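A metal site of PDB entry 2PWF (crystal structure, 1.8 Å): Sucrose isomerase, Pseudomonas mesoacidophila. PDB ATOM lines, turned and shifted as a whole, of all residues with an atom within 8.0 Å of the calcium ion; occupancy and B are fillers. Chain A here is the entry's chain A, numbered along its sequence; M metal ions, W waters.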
ATOM      1  N   PRO A  16      -3.629 -33.189   2.256  1.00  0.00           N
ATOM      2  CA  PRO A  16      -2.629 -32.168   2.640  1.00  0.00           C
ATOM      3  C   PRO A  16      -2.356 -30.974   1.763  1.00  0.00           C
ATOM      4  O   PRO A  16      -2.187 -29.888   2.248  1.00  0.00           O
ATOM      5  CB  PRO A  16      -1.351 -32.984   2.918  1.00  0.00           C
ATOM      6  CG  PRO A  16      -1.933 -34.366   3.310  1.00  0.00           C
ATOM      7  CD  PRO A  16      -3.020 -34.534   2.252  1.00  0.00           C
ATOM      8  N   ARG A  17      -2.285 -31.257   0.464  1.00  0.00           N
ATOM      9  CA  ARG A  17      -1.990 -30.286  -0.562  1.00  0.00           C
ATOM     10  C   ARG A  17      -2.913 -29.083  -0.454  1.00  0.00           C
ATOM     11  O   ARG A  17      -2.510 -27.941  -0.714  1.00  0.00           O
ATOM     12  CB  ARG A  17      -2.152 -30.975  -1.922  1.00  0.00           C
ATOM     13  CG  ARG A  17      -1.609 -30.209  -3.034  1.00  0.00           C
ATOM     14  CD  ARG A  17      -1.766 -30.976  -4.351  1.00  0.00           C
ATOM     15  NE  ARG A  17      -1.351 -30.070  -5.385  1.00  0.00           N
ATOM     16  CZ  ARG A  17      -0.100 -29.927  -5.790  1.00  0.00           C
ATOM     17  NH1 ARG A  17       0.862 -30.682  -5.268  1.00  0.00           N
ATOM     18  NH2 ARG A  17       0.204 -28.935  -6.622  1.00  0.00           N
ATOM     19  N   LYS A  20      -3.661 -26.763   4.707  1.00  0.00           N
ATOM     20  CA  LYS A  20      -3.098 -25.544   5.270  1.00  0.00           C
ATOM     21  C   LYS A  20      -1.616 -25.383   4.866  1.00  0.00           C
ATOM     22  O   LYS A  20      -0.796 -26.293   5.060  1.00  0.00           O
ATOM     23  CB  LYS A  20      -3.243 -25.561   6.810  1.00  0.00           C
ATOM     24  CG  LYS A  20      -2.651 -24.330   7.537  1.00  0.00           C
ATOM     25  CD  LYS A  20      -3.350 -23.031   7.139  1.00  0.00           C
ATOM     26  CE  LYS A  20      -3.050 -21.857   8.120  1.00  0.00           C
ATOM     27  NZ  LYS A  20      -1.590 -21.610   8.315  1.00  0.00           N
ATOM     28  N   ASP A  21      -1.293 -24.249   4.265  1.00  0.00           N
ATOM     29  CA  ASP A  21       0.065 -23.943   3.827  1.00  0.00           C
ATOM     30  C   ASP A  21       0.683 -22.975   4.848  1.00  0.00           C
ATOM     31  O   ASP A  21       0.065 -21.957   5.188  1.00  0.00           O
ATOM     32  CB  ASP A  21       0.008 -23.291   2.429  1.00  0.00           C
ATOM     33  CG  ASP A  21       1.348 -22.723   1.977  1.00  0.00           C
ATOM     34  OD1 ASP A  21       2.397 -23.215   2.407  1.00  0.00           O
ATOM     35  OD2 ASP A  21       1.333 -21.779   1.148  1.00  0.00           O
ATOM     36  N   THR A  22       1.885 -23.287   5.319  1.00  0.00           N
ATOM     37  CA  THR A  22       2.553 -22.470   6.338  1.00  0.00           C
ATOM     38  C   THR A  22       3.816 -21.749   5.837  1.00  0.00           C
ATOM     39  O   THR A  22       4.506 -21.069   6.612  1.00  0.00           O
ATOM     40  CB  THR A  22       2.906 -23.369   7.547  1.00  0.00           C
ATOM     41  OG1 THR A  22       3.720 -24.487   7.117  1.00  0.00           O
ATOM     42  CG2 THR A  22       1.597 -23.909   8.200  1.00  0.00           C
ATOM     43  N   ASN A  23       4.142 -21.883   4.558  1.00  0.00           N
ATOM     44  CA  ASN A  23       5.347 -21.227   4.062  1.00  0.00           C
ATOM     45  C   ASN A  23       5.108 -20.477   2.756  1.00  0.00           C
ATOM     46  O   ASN A  23       6.051 -20.221   2.023  1.00  0.00           O
ATOM     47  CB  ASN A  23       6.474 -22.251   3.890  1.00  0.00           C
ATOM     48  CG  ASN A  23       6.290 -23.099   2.663  1.00  0.00           C
ATOM     49  OD1 ASN A  23       5.164 -23.418   2.307  1.00  0.00           O
ATOM     50  ND2 ASN A  23       7.394 -23.466   1.995  1.00  0.00           N
ATOM     51  N   GLY A  24       3.841 -20.170   2.455  1.00  0.00           N
ATOM     52  CA  GLY A  24       3.478 -19.388   1.291  1.00  0.00           C
ATOM     53  C   GLY A  24       3.777 -19.848  -0.116  1.00  0.00           C
ATOM     54  O   GLY A  24       3.762 -19.025  -1.032  1.00  0.00           O
ATOM     55  N   ASP A  25       4.078 -21.120  -0.310  1.00  0.00           N
ATOM     56  CA  ASP A  25       4.320 -21.599  -1.670  1.00  0.00           C
ATOM     57  C   ASP A  25       2.968 -21.970  -2.308  1.00  0.00           C
ATOM     58  O   ASP A  25       2.931 -22.413  -3.454  1.00  0.00           O
ATOM     59  CB  ASP A  25       5.307 -22.778  -1.669  1.00  0.00           C
ATOM     60  CG  ASP A  25       4.715 -24.048  -1.039  1.00  0.00           C
ATOM     61  OD1 ASP A  25       3.676 -23.995  -0.355  1.00  0.00           O
ATOM     62  OD2 ASP A  25       5.361 -25.111  -1.236  1.00  0.00           O
ATOM     63  N   GLY A  26       1.878 -21.761  -1.578  1.00  0.00           N
ATOM     64  CA  GLY A  26       0.534 -22.079  -2.095  1.00  0.00           C
ATOM     65  C   GLY A  26       0.136 -23.545  -2.011  1.00  0.00           C
ATOM     66  O   GLY A  26      -0.886 -23.972  -2.591  1.00  0.00           O
ATOM     67  N   ILE A  27       0.923 -24.344  -1.287  1.00  0.00           N
ATOM     68  CA  ILE A  27       0.604 -25.786  -1.166  1.00  0.00           C
ATOM     69  C   ILE A  27       0.619 -26.168   0.309  1.00  0.00           C
ATOM     70  O   ILE A  27       1.583 -25.841   1.040  1.00  0.00           O
ATOM     71  CB  ILE A  27       1.630 -26.646  -1.947  1.00  0.00           C
ATOM     72  CG1 ILE A  27       1.531 -26.352  -3.463  1.00  0.00           C
ATOM     73  CG2 ILE A  27       1.424 -28.153  -1.616  1.00  0.00           C
ATOM     74  CD1 ILE A  27       2.714 -26.936  -4.268  1.00  0.00           C
ATOM     75  N   GLY A  28      -0.445 -26.838   0.750  1.00  0.00           N
ATOM     76  CA  GLY A  28      -0.534 -27.261   2.150  1.00  0.00           C
ATOM     77  C   GLY A  28       0.624 -28.174   2.525  1.00  0.00           C
ATOM     78  O   GLY A  28       1.267 -28.791   1.662  1.00  0.00           O
ATOM     79  N   ASP A  29       0.888 -28.281   3.810  1.00  0.00           N
ATOM     80  CA  ASP A  29       2.023 -29.080   4.263  1.00  0.00           C
ATOM     81  C   ASP A  29       1.748 -29.666   5.656  1.00  0.00           C
ATOM     82  O   ASP A  29       0.731 -29.380   6.288  1.00  0.00           O
ATOM     83  CB  ASP A  29       3.251 -28.180   4.269  1.00  0.00           C
ATOM     84  CG  ASP A  29       2.940 -26.771   4.831  1.00  0.00           C
ATOM     85  OD1 ASP A  29       2.661 -26.651   6.049  1.00  0.00           O
ATOM     86  OD2 ASP A  29       2.967 -25.802   4.036  1.00  0.00           O
ATOM     87  N   PHE A  30       2.696 -30.476   6.117  1.00  0.00           N
ATOM     88  CA  PHE A  30       2.594 -31.146   7.408  1.00  0.00           C
ATOM     89  C   PHE A  30       2.502 -30.177   8.558  1.00  0.00           C
ATOM     90  O   PHE A  30       1.762 -30.427   9.494  1.00  0.00           O
ATOM     91  CB  PHE A  30       3.807 -32.053   7.623  1.00  0.00           C
ATOM     92  CG  PHE A  30       3.800 -33.283   6.772  1.00  0.00           C
ATOM     93  CD1 PHE A  30       2.636 -34.018   6.581  1.00  0.00           C
ATOM     94  CD2 PHE A  30       4.986 -33.753   6.217  1.00  0.00           C
ATOM     95  CE1 PHE A  30       2.639 -35.214   5.865  1.00  0.00           C
ATOM     96  CE2 PHE A  30       5.006 -34.940   5.495  1.00  0.00           C
ATOM     97  CZ  PHE A  30       3.815 -35.676   5.328  1.00  0.00           C
ATOM     98  N   LYS A  31       3.297 -29.109   8.544  1.00  0.00           N
ATOM     99  CA  LYS A  31       3.210 -28.139   9.632  1.00  0.00           C
ATOM    100  C   LYS A  31       1.839 -27.475   9.699  1.00  0.00           C
ATOM    101  O   LYS A  31       1.380 -27.114  10.775  1.00  0.00           O
ATOM    102  CB  LYS A  31       4.284 -27.057   9.490  1.00  0.00           C
ATOM    103  CG  LYS A  31       5.660 -27.543   9.909  1.00  0.00           C
ATOM    104  CD  LYS A  31       6.661 -26.404   9.894  1.00  0.00           C
ATOM    105  CE  LYS A  31       8.075 -26.955  10.093  1.00  0.00           C
ATOM    106  NZ  LYS A  31       9.083 -25.882   9.905  1.00  0.00           N
ATOM    107  N   GLY A  32       1.170 -27.305   8.553  1.00  0.00           N
ATOM    108  CA  GLY A  32      -0.136 -26.672   8.633  1.00  0.00           C
ATOM    109  C   GLY A  32      -1.134 -27.625   9.226  1.00  0.00           C
ATOM    110  O   GLY A  32      -1.967 -27.258  10.045  1.00  0.00           O
ATOM    111  N   LYS A  73       8.660 -33.620  -0.689  1.00  0.00           N
ATOM    112  CA  LYS A  73       9.363 -32.366  -0.424  1.00  0.00           C
ATOM    113  C   LYS A  73       8.401 -31.229  -0.040  1.00  0.00           C
ATOM    114  O   LYS A  73       8.641 -30.507   0.923  1.00  0.00           O
ATOM    115  CB  LYS A  73      10.207 -32.009  -1.660  1.00  0.00           C
ATOM    116  N   GLU A  74       7.313 -31.100  -0.791  1.00  0.00           N
ATOM    117  CA  GLU A  74       6.335 -30.044  -0.523  1.00  0.00           C
ATOM    118  C   GLU A  74       5.704 -30.066   0.871  1.00  0.00           C
ATOM    119  O   GLU A  74       5.342 -29.024   1.429  1.00  0.00           O
ATOM    120  CB  GLU A  74       5.191 -30.107  -1.559  1.00  0.00           C
ATOM    121  CG  GLU A  74       5.513 -29.489  -2.935  1.00  0.00           C
ATOM    122  CD  GLU A  74       6.274 -30.446  -3.847  1.00  0.00           C
ATOM    123  OE1 GLU A  74       6.471 -31.611  -3.450  1.00  0.00           O
ATOM    124  OE2 GLU A  74       6.656 -30.037  -4.964  1.00  0.00           O
ATOM    125  N   TYR A  75       5.525 -31.262   1.425  1.00  0.00           N
ATOM    126  CA  TYR A  75       4.883 -31.379   2.738  1.00  0.00           C
ATOM    127  C   TYR A  75       5.809 -31.165   3.913  1.00  0.00           C
ATOM    128  O   TYR A  75       5.354 -30.870   5.011  1.00  0.00           O
ATOM    129  CB  TYR A  75       4.154 -32.723   2.876  1.00  0.00           C
ATOM    130  CG  TYR A  75       3.041 -32.905   1.863  1.00  0.00           C
ATOM    131  CD1 TYR A  75       2.646 -31.851   1.020  1.00  0.00           C
ATOM    132  CD2 TYR A  75       2.416 -34.142   1.700  1.00  0.00           C
ATOM    133  CE1 TYR A  75       1.667 -32.036   0.030  1.00  0.00           C
ATOM    134  CE2 TYR A  75       1.446 -34.330   0.737  1.00  0.00           C
ATOM    135  CZ  TYR A  75       1.070 -33.292  -0.106  1.00  0.00           C
ATOM    136  OH  TYR A  75       0.148 -33.530  -1.105  1.00  0.00           O
ATOM    137  N   GLY A  76       7.101 -31.272   3.672  1.00  0.00           N
ATOM    138  CA  GLY A  76       8.056 -31.078   4.753  1.00  0.00           C
ATOM    139  C   GLY A  76       9.078 -32.182   4.764  1.00  0.00           C
ATOM    140  O   GLY A  76       9.399 -32.771   3.741  1.00  0.00           O
ATOM    141  N   PHE A 430      -5.860 -19.940   3.850  1.00  0.00           N
ATOM    142  CA  PHE A 430      -5.151 -21.169   3.466  1.00  0.00           C
ATOM    143  C   PHE A 430      -3.679 -20.868   3.221  1.00  0.00           C
ATOM    144  O   PHE A 430      -2.828 -21.678   3.542  1.00  0.00           O
ATOM    145  CB  PHE A 430      -5.730 -21.717   2.167  1.00  0.00           C
ATOM    146  CG  PHE A 430      -4.855 -22.769   1.500  1.00  0.00           C
ATOM    147  CD1 PHE A 430      -4.659 -24.023   2.105  1.00  0.00           C
ATOM    148  CD2 PHE A 430      -4.269 -22.515   0.271  1.00  0.00           C
ATOM    149  CE1 PHE A 430      -3.883 -25.004   1.491  1.00  0.00           C
ATOM    150  CE2 PHE A 430      -3.468 -23.517  -0.375  1.00  0.00           C
ATOM    151  CZ  PHE A 430      -3.282 -24.764   0.249  1.00  0.00           C
ATOM    152  N   THR A 431      -3.368 -19.699   2.681  1.00  0.00           N
ATOM    153  CA  THR A 431      -1.977 -19.398   2.358  1.00  0.00           C
ATOM    154  C   THR A 431      -1.742 -17.892   2.249  1.00  0.00           C
ATOM    155  O   THR A 431      -2.690 -17.124   1.964  1.00  0.00           O
ATOM    156  CB  THR A 431      -1.608 -20.026   0.986  1.00  0.00           C
ATOM    157  OG1 THR A 431      -0.254 -19.706   0.647  1.00  0.00           O
ATOM    158  CG2 THR A 431      -2.541 -19.463  -0.132  1.00  0.00           C
HETATM  159 CA    CA M   1       3.611 -25.009   1.861  1.00  0.00          CA
HETATM  160  O   HOH W   1       4.512 -26.778   0.449  1.00  0.00           O
HETATM  161  O   HOH W   2       5.646 -26.285   2.809  1.00  0.00           O
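The calcium ion is bound by the side-chain carboxylate (OD1) of Asp 21, the side-chain amide oxygen (OD1) of Asn 23, the backbone carbonyl oxygen (O) of Ile 27, the side-chain carboxylate (OD2) of Asp 29, water W1, the side-chain carboxylate (OD1) of Asp 25 and water W2.
Water W1 lies within hydrogen-bond range of the side-chain carboxylate (OD2) of Asp 25 and the backbone carbonyl oxygen (O) of Glu 74.
Water W2 lies within hydrogen-bond range of the backbone carbonyl oxygen of Glu 74 (3.1 Å) and the side-chain amide nitrogen of Asn 23 (3.4 Å).
The backbone NH (N) of Gly 26 sits at hydrogen-bond distance from the side-chain carboxylate (OD2) of Asp 21.
The backbone NH of Gly 24 sits close to the side-chain carboxylate of Asp 21 (3.3 Å).
The side-chain carboxylate (OD1) of Asp 29 lies within hydrogen-bond range of the side-chain hydroxyl (OG1) of Thr 22, at 2.6 Å.
OG1 of Thr 431 is in hydrogen-bond range of OD2 of Asp 21 (2.7 Å).
The backbone NH of Asp 29 lies within hydrogen-bond range of the backbone carbonyl oxygen of Lys 20 (2.9 Å).
The backbone NH of Asp 21 lies within hydrogen-bond range of the backbone carbonyl oxygen of Phe 430 (3.1 Å).
OD1 of Asp 29 is in hydrogen-bond range of N of Gly 32 (3.0 Å).
The nearest printed residue that does not touch the calcium ion is Thr 22 (4.2 Å).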
